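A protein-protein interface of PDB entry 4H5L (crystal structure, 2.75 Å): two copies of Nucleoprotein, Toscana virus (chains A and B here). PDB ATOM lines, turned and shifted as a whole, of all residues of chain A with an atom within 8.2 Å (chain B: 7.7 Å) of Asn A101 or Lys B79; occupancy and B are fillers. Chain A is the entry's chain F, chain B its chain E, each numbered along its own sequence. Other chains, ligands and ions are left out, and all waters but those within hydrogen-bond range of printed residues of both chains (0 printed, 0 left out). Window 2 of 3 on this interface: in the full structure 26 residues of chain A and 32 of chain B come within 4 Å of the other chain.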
ATOM      1  N   GLU A  29      41.783  21.507  10.476  1.00  0.00           N
ATOM      2  CA  GLU A  29      41.183  20.603   9.496  1.00  0.00           C
ATOM      3  C   GLU A  29      40.179  19.619  10.137  1.00  0.00           C
ATOM      4  O   GLU A  29      39.244  19.187   9.463  1.00  0.00           O
ATOM      5  CB  GLU A  29      42.272  19.834   8.739  1.00  0.00           C
ATOM      6  CG  GLU A  29      41.870  19.417   7.332  1.00  0.00           C
ATOM      7  CD  GLU A  29      41.605  20.546   6.344  1.00  0.00           C
ATOM      8  OE1 GLU A  29      42.591  21.112   5.813  1.00  0.00           O
ATOM      9  OE2 GLU A  29      40.415  20.862   6.098  1.00  0.00           O
ATOM     10  N   PHE A  30      40.356  19.284  11.429  1.00  0.00           N
ATOM     11  CA  PHE A  30      39.488  18.345  12.148  1.00  0.00           C
ATOM     12  C   PHE A  30      38.373  19.014  12.973  1.00  0.00           C
ATOM     13  O   PHE A  30      37.395  18.332  13.288  1.00  0.00           O
ATOM     14  CB  PHE A  30      40.320  17.439  13.081  1.00  0.00           C
ATOM     15  CG  PHE A  30      41.256  16.455  12.421  1.00  0.00           C
ATOM     16  CD1 PHE A  30      40.896  15.807  11.243  1.00  0.00           C
ATOM     17  CD2 PHE A  30      42.461  16.115  13.017  1.00  0.00           C
ATOM     18  CE1 PHE A  30      41.752  14.873  10.650  1.00  0.00           C
ATOM     19  CE2 PHE A  30      43.315  15.180  12.425  1.00  0.00           C
ATOM     20  CZ  PHE A  30      42.957  14.568  11.244  1.00  0.00           C
ATOM     21  N   ALA A  31      38.513  20.327  13.309  1.00  0.00           N
ATOM     22  CA  ALA A  31      37.585  21.128  14.134  1.00  0.00           C
ATOM     23  C   ALA A  31      36.116  21.036  13.704  1.00  0.00           C
ATOM     24  O   ALA A  31      35.824  20.759  12.535  1.00  0.00           O
ATOM     25  CB  ALA A  31      38.010  22.588  14.132  1.00  0.00           C
ATOM     26  N   TYR A  32      35.195  21.299  14.663  1.00  0.00           N
ATOM     27  CA  TYR A  32      33.746  21.280  14.439  1.00  0.00           C
ATOM     28  C   TYR A  32      33.346  22.336  13.411  1.00  0.00           C
ATOM     29  O   TYR A  32      33.653  23.520  13.575  1.00  0.00           O
ATOM     30  CB  TYR A  32      32.963  21.492  15.749  1.00  0.00           C
ATOM     31  CG  TYR A  32      31.469  21.286  15.594  1.00  0.00           C
ATOM     32  CD1 TYR A  32      30.892  20.037  15.804  1.00  0.00           C
ATOM     33  CD2 TYR A  32      30.634  22.338  15.221  1.00  0.00           C
ATOM     34  CE1 TYR A  32      29.520  19.843  15.667  1.00  0.00           C
ATOM     35  CE2 TYR A  32      29.263  22.149  15.058  1.00  0.00           C
ATOM     36  CZ  TYR A  32      28.708  20.899  15.282  1.00  0.00           C
ATOM     37  OH  TYR A  32      27.353  20.709  15.146  1.00  0.00           O
ATOM     38  N   GLN A  33      32.645  21.891  12.364  1.00  0.00           N
ATOM     39  CA  GLN A  33      32.182  22.722  11.255  1.00  0.00           C
ATOM     40  C   GLN A  33      30.799  22.208  10.814  1.00  0.00           C
ATOM     41  O   GLN A  33      30.704  21.154  10.178  1.00  0.00           O
ATOM     42  CB  GLN A  33      33.229  22.666  10.118  1.00  0.00           C
ATOM     43  CG  GLN A  33      32.990  23.615   8.956  1.00  0.00           C
ATOM     44  CD  GLN A  33      33.229  22.921   7.628  1.00  0.00           C
ATOM     45  OE1 GLN A  33      32.389  22.146   7.133  1.00  0.00           O
ATOM     46  NE2 GLN A  33      34.386  23.179   7.024  1.00  0.00           N
ATOM     47  N   GLY A  34      29.743  22.933  11.191  1.00  0.00           N
ATOM     48  CA  GLY A  34      28.370  22.554  10.864  1.00  0.00           C
ATOM     49  C   GLY A  34      28.060  22.546   9.377  1.00  0.00           C
ATOM     50  O   GLY A  34      27.334  21.681   8.879  1.00  0.00           O
ATOM     51  N   PHE A  35      28.655  23.509   8.672  1.00  0.00           N
ATOM     52  CA  PHE A  35      28.524  23.808   7.250  1.00  0.00           C
ATOM     53  C   PHE A  35      29.668  24.737   6.823  1.00  0.00           C
ATOM     54  O   PHE A  35      30.277  25.398   7.677  1.00  0.00           O
ATOM     55  CB  PHE A  35      27.154  24.486   6.982  1.00  0.00           C
ATOM     56  CG  PHE A  35      27.013  25.884   7.545  1.00  0.00           C
ATOM     57  CD1 PHE A  35      27.158  26.998   6.726  1.00  0.00           C
ATOM     58  CD2 PHE A  35      26.742  26.085   8.893  1.00  0.00           C
ATOM     59  CE1 PHE A  35      27.048  28.291   7.250  1.00  0.00           C
ATOM     60  CE2 PHE A  35      26.626  27.376   9.414  1.00  0.00           C
ATOM     61  CZ  PHE A  35      26.783  28.470   8.592  1.00  0.00           C
ATOM     62  N   ASN A  71      13.341  27.754  10.626  1.00  0.00           N
ATOM     63  CA  ASN A  71      14.175  26.973   9.711  1.00  0.00           C
ATOM     64  C   ASN A  71      13.454  25.737   9.114  1.00  0.00           C
ATOM     65  O   ASN A  71      14.110  24.832   8.579  1.00  0.00           O
ATOM     66  CB  ASN A  71      15.447  26.544  10.447  1.00  0.00           C
ATOM     67  CG  ASN A  71      16.657  26.396   9.567  1.00  0.00           C
ATOM     68  OD1 ASN A  71      16.829  27.108   8.570  1.00  0.00           O
ATOM     69  ND2 ASN A  71      17.551  25.483   9.940  1.00  0.00           N
ATOM     70  N   LYS A  98      16.355  22.747   2.873  1.00  0.00           N
ATOM     71  CA  LYS A  98      16.051  21.653   3.784  1.00  0.00           C
ATOM     72  C   LYS A  98      15.827  22.187   5.209  1.00  0.00           C
ATOM     73  O   LYS A  98      15.925  23.399   5.445  1.00  0.00           O
ATOM     74  CB  LYS A  98      17.171  20.600   3.744  1.00  0.00           C
ATOM     75  CG  LYS A  98      16.757  19.285   3.091  1.00  0.00           C
ATOM     76  CD  LYS A  98      16.857  19.325   1.574  1.00  0.00           C
ATOM     77  CE  LYS A  98      16.085  18.195   0.940  1.00  0.00           C
ATOM     78  NZ  LYS A  98      15.989  18.359  -0.535  1.00  0.00           N
ATOM     79  N   GLU A  99      15.488  21.280   6.142  1.00  0.00           N
ATOM     80  CA  GLU A  99      15.213  21.596   7.549  1.00  0.00           C
ATOM     81  C   GLU A  99      16.367  21.149   8.451  1.00  0.00           C
ATOM     82  O   GLU A  99      17.200  20.336   8.034  1.00  0.00           O
ATOM     83  CB  GLU A  99      13.899  20.931   8.013  1.00  0.00           C
ATOM     84  CG  GLU A  99      12.684  21.296   7.171  1.00  0.00           C
ATOM     85  CD  GLU A  99      11.319  20.849   7.668  1.00  0.00           C
ATOM     86  OE1 GLU A  99      11.262  19.989   8.580  1.00  0.00           O
ATOM     87  OE2 GLU A  99      10.305  21.355   7.127  1.00  0.00           O
ATOM     88  N   GLY A 100      16.385  21.682   9.674  1.00  0.00           N
ATOM     89  CA  GLY A 100      17.357  21.345  10.709  1.00  0.00           C
ATOM     90  C   GLY A 100      18.820  21.553  10.377  1.00  0.00           C
ATOM     91  O   GLY A 100      19.196  22.626   9.895  1.00  0.00           O
ATOM     92  N   ASN A 101      19.654  20.524  10.657  1.00  0.00           N
ATOM     93  CA  ASN A 101      21.100  20.584  10.446  1.00  0.00           C
ATOM     94  C   ASN A 101      21.593  19.414   9.563  1.00  0.00           C
ATOM     95  O   ASN A 101      22.091  18.413  10.087  1.00  0.00           O
ATOM     96  CB  ASN A 101      21.832  20.614  11.801  1.00  0.00           C
ATOM     97  CG  ASN A 101      23.108  21.431  11.837  1.00  0.00           C
ATOM     98  OD1 ASN A 101      23.412  22.240  10.943  1.00  0.00           O
ATOM     99  ND2 ASN A 101      23.869  21.264  12.910  1.00  0.00           N
ATOM    100  N   PRO A 102      21.494  19.534   8.216  1.00  0.00           N
ATOM    101  CA  PRO A 102      21.959  18.445   7.344  1.00  0.00           C
ATOM    102  C   PRO A 102      23.442  18.585   6.944  1.00  0.00           C
ATOM    103  O   PRO A 102      24.233  19.151   7.699  1.00  0.00           O
ATOM    104  CB  PRO A 102      21.021  18.550   6.139  1.00  0.00           C
ATOM    105  CG  PRO A 102      20.512  19.972   6.156  1.00  0.00           C
ATOM    106  CD  PRO A 102      20.923  20.639   7.425  1.00  0.00           C
ATOM    107  N   GLY A 103      23.800  18.047   5.775  1.00  0.00           N
ATOM    108  CA  GLY A 103      25.157  18.056   5.233  1.00  0.00           C
ATOM    109  C   GLY A 103      25.703  19.417   4.844  1.00  0.00           C
ATOM    110  O   GLY A 103      24.948  20.379   4.703  1.00  0.00           O
ATOM    111  N   ARG A 104      27.035  19.482   4.642  1.00  0.00           N
ATOM    112  CA  ARG A 104      27.828  20.666   4.271  1.00  0.00           C
ATOM    113  C   ARG A 104      27.421  21.329   2.945  1.00  0.00           C
ATOM    114  O   ARG A 104      27.688  22.523   2.769  1.00  0.00           O
ATOM    115  CB  ARG A 104      29.300  20.276   4.143  1.00  0.00           C
ATOM    116  CG  ARG A 104      30.146  20.539   5.363  1.00  0.00           C
ATOM    117  CD  ARG A 104      31.577  20.143   5.063  1.00  0.00           C
ATOM    118  NE  ARG A 104      31.792  18.699   5.226  1.00  0.00           N
ATOM    119  CZ  ARG A 104      31.912  17.832   4.225  1.00  0.00           C
ATOM    120  NH1 ARG A 104      31.843  18.247   2.965  1.00  0.00           N
ATOM    121  NH2 ARG A 104      32.098  16.544   4.475  1.00  0.00           N
ATOM    122  N   THR A 106      24.251  21.356   1.784  1.00  0.00           N
ATOM    123  CA  THR A 106      22.815  21.602   1.857  1.00  0.00           C
ATOM    124  C   THR A 106      22.561  23.015   2.388  1.00  0.00           C
ATOM    125  O   THR A 106      23.166  23.416   3.381  1.00  0.00           O
ATOM    126  CB  THR A 106      22.127  20.530   2.701  1.00  0.00           C
ATOM    127  OG1 THR A 106      22.726  19.255   2.447  1.00  0.00           O
ATOM    128  CG2 THR A 106      20.647  20.456   2.422  1.00  0.00           C
ATOM    129  N   THR A 108      20.113  25.863   4.115  1.00  0.00           N
ATOM    130  CA  THR A 108      18.999  26.056   5.051  1.00  0.00           C
ATOM    131  C   THR A 108      18.842  27.551   5.300  1.00  0.00           C
ATOM    132  O   THR A 108      19.816  28.291   5.173  1.00  0.00           O
ATOM    133  CB  THR A 108      19.151  25.277   6.368  1.00  0.00           C
ATOM    134  OG1 THR A 108      20.039  25.931   7.269  1.00  0.00           O
ATOM    135  CG2 THR A 108      19.488  23.820   6.186  1.00  0.00           C
ATOM    136  N   SER A 110      18.587  29.154   8.117  1.00  0.00           N
ATOM    137  CA  SER A 110      19.521  29.517   9.191  1.00  0.00           C
ATOM    138  C   SER A 110      20.952  29.713   8.670  1.00  0.00           C
ATOM    139  O   SER A 110      21.662  30.601   9.155  1.00  0.00           O
ATOM    140  CB  SER A 110      19.519  28.469  10.298  1.00  0.00           C
ATOM    141  OG  SER A 110      18.383  28.588  11.140  1.00  0.00           O
ATOM    142  N   ARG A 111      21.363  28.900   7.680  1.00  0.00           N
ATOM    143  CA  ARG A 111      22.699  28.975   7.097  1.00  0.00           C
ATOM    144  C   ARG A 111      22.866  30.235   6.235  1.00  0.00           C
ATOM    145  O   ARG A 111      23.915  30.888   6.311  1.00  0.00           O
ATOM    146  CB  ARG A 111      23.011  27.708   6.305  1.00  0.00           C
ATOM    147  CG  ARG A 111      23.387  26.561   7.225  1.00  0.00           C
ATOM    148  CD  ARG A 111      23.411  25.219   6.535  1.00  0.00           C
ATOM    149  NE  ARG A 111      23.607  24.139   7.502  1.00  0.00           N
ATOM    150  CZ  ARG A 111      23.872  22.883   7.176  1.00  0.00           C
ATOM    151  NH1 ARG A 111      23.994  22.533   5.902  1.00  0.00           N
ATOM    152  NH2 ARG A 111      24.033  21.966   8.120  1.00  0.00           N
ATOM    153  N   PRO A 205      28.301  24.909  19.198  1.00  0.00           N
ATOM    154  CA  PRO A 205      28.188  25.478  17.837  1.00  0.00           C
ATOM    155  C   PRO A 205      28.469  26.987  17.758  1.00  0.00           C
ATOM    156  O   PRO A 205      28.931  27.445  16.710  1.00  0.00           O
ATOM    157  CB  PRO A 205      26.739  25.177  17.441  1.00  0.00           C
ATOM    158  CG  PRO A 205      26.260  24.150  18.417  1.00  0.00           C
ATOM    159  CD  PRO A 205      26.982  24.454  19.681  1.00  0.00           C
ATOM    160  N   ALA A 208      32.295  27.456  17.773  1.00  0.00           N
ATOM    161  CA  ALA A 208      32.755  27.058  16.442  1.00  0.00           C
ATOM    162  C   ALA A 208      32.504  28.170  15.426  1.00  0.00           C
ATOM    163  O   ALA A 208      33.305  28.347  14.505  1.00  0.00           O
ATOM    164  CB  ALA A 208      32.045  25.784  16.007  1.00  0.00           C
ATOM    165  N   ARG B  69      38.037  16.152  19.007  1.00  0.00           N
ATOM    166  CA  ARG B  69      36.696  15.803  18.529  1.00  0.00           C
ATOM    167  C   ARG B  69      35.993  14.620  19.242  1.00  0.00           C
ATOM    168  O   ARG B  69      34.800  14.401  18.994  1.00  0.00           O
ATOM    169  CB  ARG B  69      36.712  15.552  17.009  1.00  0.00           C
ATOM    170  CG  ARG B  69      36.937  16.811  16.166  1.00  0.00           C
ATOM    171  CD  ARG B  69      35.798  17.834  16.240  1.00  0.00           C
ATOM    172  NE  ARG B  69      34.947  17.775  15.058  1.00  0.00           N
ATOM    173  CZ  ARG B  69      33.735  17.238  15.038  1.00  0.00           C
ATOM    174  NH1 ARG B  69      33.203  16.740  16.147  1.00  0.00           N
ATOM    175  NH2 ARG B  69      33.040  17.206  13.913  1.00  0.00           N
ATOM    176  N   GLU B  74      32.533   8.136  13.297  1.00  0.00           N
ATOM    177  CA  GLU B  74      31.461   8.208  12.308  1.00  0.00           C
ATOM    178  C   GLU B  74      30.666   9.522  12.442  1.00  0.00           C
ATOM    179  O   GLU B  74      30.379  10.173  11.433  1.00  0.00           O
ATOM    180  CB  GLU B  74      30.527   7.003  12.466  1.00  0.00           C
ATOM    181  CG  GLU B  74      29.806   6.614  11.185  1.00  0.00           C
ATOM    182  CD  GLU B  74      30.652   5.949  10.113  1.00  0.00           C
ATOM    183  OE1 GLU B  74      31.470   5.067  10.463  1.00  0.00           O
ATOM    184  OE2 GLU B  74      30.472   6.288   8.920  1.00  0.00           O
ATOM    185  N   ALA B  75      30.352   9.914  13.693  1.00  0.00           N
ATOM    186  CA  ALA B  75      29.585  11.108  14.039  1.00  0.00           C
ATOM    187  C   ALA B  75      30.329  12.414  13.751  1.00  0.00           C
ATOM    188  O   ALA B  75      29.709  13.356  13.253  1.00  0.00           O
ATOM    189  CB  ALA B  75      29.188  11.066  15.506  1.00  0.00           C
ATOM    190  N   MET B  76      31.633  12.489  14.092  1.00  0.00           N
ATOM    191  CA  MET B  76      32.455  13.696  13.914  1.00  0.00           C
ATOM    192  C   MET B  76      32.725  14.015  12.433  1.00  0.00           C
ATOM    193  O   MET B  76      33.032  15.164  12.117  1.00  0.00           O
ATOM    194  CB  MET B  76      33.788  13.602  14.698  1.00  0.00           C
ATOM    195  CG  MET B  76      34.704  12.443  14.278  1.00  0.00           C
ATOM    196  SD  MET B  76      36.282  12.333  15.180  1.00  0.00           S
ATOM    197  CE  MET B  76      35.703  11.937  16.851  1.00  0.00           C
ATOM    198  N   MET B  77      32.615  13.006  11.544  1.00  0.00           N
ATOM    199  CA  MET B  77      32.827  13.130  10.108  1.00  0.00           C
ATOM    200  C   MET B  77      31.816  14.067   9.444  1.00  0.00           C
ATOM    201  O   MET B  77      32.202  14.864   8.590  1.00  0.00           O
ATOM    202  CB  MET B  77      32.725  11.756   9.464  1.00  0.00           C
ATOM    203  CG  MET B  77      34.046  11.090   9.259  1.00  0.00           C
ATOM    204  SD  MET B  77      33.844   9.617   8.239  1.00  0.00           S
ATOM    205  CE  MET B  77      33.719  10.351   6.634  1.00  0.00           C
ATOM    206  N   LYS B  78      30.525  13.958   9.832  1.00  0.00           N
ATOM    207  CA  LYS B  78      29.387  14.727   9.311  1.00  0.00           C
ATOM    208  C   LYS B  78      29.526  16.233   9.557  1.00  0.00           C
ATOM    209  O   LYS B  78      29.113  17.026   8.708  1.00  0.00           O
ATOM    210  CB  LYS B  78      28.072  14.221   9.931  1.00  0.00           C
ATOM    211  CG  LYS B  78      27.648  12.836   9.430  1.00  0.00           C
ATOM    212  CD  LYS B  78      27.375  11.844  10.566  1.00  0.00           C
ATOM    213  CE  LYS B  78      25.918  11.762  10.962  1.00  0.00           C
ATOM    214  NZ  LYS B  78      25.703  10.783  12.059  1.00  0.00           N
ATOM    215  N   LYS B  79      30.103  16.621  10.705  1.00  0.00           N
ATOM    216  CA  LYS B  79      30.293  18.021  11.082  1.00  0.00           C
ATOM    217  C   LYS B  79      31.786  18.396  11.011  1.00  0.00           C
ATOM    218  O   LYS B  79      32.353  18.903  11.978  1.00  0.00           O
ATOM    219  CB  LYS B  79      29.708  18.294  12.484  1.00  0.00           C
ATOM    220  CG  LYS B  79      28.258  17.858  12.679  1.00  0.00           C
ATOM    221  CD  LYS B  79      27.261  18.839  12.077  1.00  0.00           C
ATOM    222  CE  LYS B  79      25.955  18.162  11.757  1.00  0.00           C
ATOM    223  NZ  LYS B  79      25.285  18.801  10.597  1.00  0.00           N
ATOM    224  N   MET B  80      32.399  18.181   9.838  1.00  0.00           N
ATOM    225  CA  MET B  80      33.818  18.434   9.584  1.00  0.00           C
ATOM    226  C   MET B  80      34.070  18.806   8.122  1.00  0.00           C
ATOM    227  O   MET B  80      33.275  18.447   7.260  1.00  0.00           O
ATOM    228  CB  MET B  80      34.608  17.154   9.924  1.00  0.00           C
ATOM    229  CG  MET B  80      36.073  17.372  10.256  1.00  0.00           C
ATOM    230  SD  MET B  80      36.943  15.788  10.343  1.00  0.00           S
ATOM    231  CE  MET B  80      36.533  15.280  11.976  1.00  0.00           C
ATOM    232  N   SER B  81      35.217  19.464   7.847  1.00  0.00           N
ATOM    233  CA  SER B  81      35.702  19.868   6.521  1.00  0.00           C
ATOM    234  C   SER B  81      35.822  18.658   5.597  1.00  0.00           C
ATOM    235  O   SER B  81      36.047  17.554   6.090  1.00  0.00           O
ATOM    236  CB  SER B  81      37.066  20.541   6.651  1.00  0.00           C
ATOM    237  OG  SER B  81      37.132  21.402   7.776  1.00  0.00           O
ATOM    238  N   ALA B  85      37.489  15.186   6.996  1.00  0.00           N
ATOM    239  CA  ALA B  85      36.614  14.004   6.995  1.00  0.00           C
ATOM    240  C   ALA B  85      37.130  12.904   6.052  1.00  0.00           C
ATOM    241  O   ALA B  85      36.829  11.736   6.274  1.00  0.00           O
ATOM    242  CB  ALA B  85      35.198  14.397   6.617  1.00  0.00           C
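O of Phe A30 sits at hydrogen-bond distance from NE of Arg B69.
The backbone carbonyl oxygen (O) of Lys B79 is in hydrogen-bond range of the backbone NH (N) of Gln A33, at 3.0 Å.
NZ of Lys B79 lies within hydrogen-bond range of O of Asn A101.
NZ of Lys B79 sits at hydrogen-bond distance from O of Pro A102, 3.1 Å away.
N of Met B80 lies within hydrogen-bond range of O of Gln A33, at 3.4 Å.
The backbone carbonyl oxygen (O) of Met B80 sits at hydrogen-bond distance from the guanidinium group (NE) of Arg A104.
The side-chain hydroxyl (OG) of Ser B81 lies within hydrogen-bond range of the backbone carbonyl oxygen (O) of Glu A29.
The side-chain hydroxyl (OG) of Ser B81 lies within hydrogen-bond range of the side-chain amide nitrogen (NE2) of Gln A33.
NH2 of Arg B69 lies within hydrogen-bond range of O of Met B76 (2.7 Å).
The guanidinium group (NH2) of Arg B69 lies within hydrogen-bond range of the backbone carbonyl oxygen (O) of Lys B79 (2.7 Å).
SD of Met B80 lies within hydrogen-bond range of N of Ala B85 (3.4 Å).
The backbone carbonyl oxygen (O) of Gly A34 is in hydrogen-bond range of the guanidinium group (NH2) of Arg A111, 3.4 Å away.
The side-chain amide oxygen of Asn A101 sits at hydrogen-bond distance from the guanidinium group of Arg A111.
The backbone carbonyl oxygen (O) of Pro A102 sits at hydrogen-bond distance from the guanidinium group (NH2) of Arg A111 (2.9 Å).
CG of Met B80 touches O of Glu A29, 3.7 Å away.
Met B80 touches Phe A30 (CE to O, 3.4 Å).
Arg B69 touches Ala A31.
Lys B79 touches Ala A31 (O to O, 3.98 Å).
N of Tyr A32 touches NE of Arg B69, 3.6 Å away.
Lys B79 touches Tyr A32 (CB to CE1, 3.5 Å).
NZ of Lys B79 touches O of Gly A34 (3.9 Å).
Of chain B, only Lys B79 comes within 4 Å of Asn A101.
Lys B79 touches six residues of chain A.
Of chain B, only Lys B79 comes within 4 Å of Pro A102.
Printed residues of chain B within 4 Å of Tyr A32: Arg B69 and Lys B79.
Printed residues of chain B within 4 Å of Glu A29: Met B80 and Ser B81.
Printed residues of chain B within 4 Å of Phe A30: Arg B69 (3.1 Å) and Met B80 (3.4 Å).
Of the printed residues of chain A, Met B80 touches Glu A29, Phe A30, Gln A33 and Arg A104.
The nearest residue of chain B that does not touch Asn A101 is Lys B78 (7.3 Å).
Of the 21 printed residues of chain A, 9 touch a printed residue of chain B.
Hydrophobic or aromatic side chains of chain A within 4 Å of the printed part of chain B: Tyr A32.
Along chain A the printed residues that touch a printed residue of chain B span positions 29 to 104.
Hydrophobic or aromatic side chains of chain B within 4 Å of the printed part of chain A: Met B80.
Among the printed residues, no Asp or Glu carboxylate lies within 4 Å of a Lys or Arg side-chain nitrogen of the other chain.
No position is printed for both chains.
Of the 15 pairs that touch across the chains among the printed residues, none has its exchanged pair printed and touching as well.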
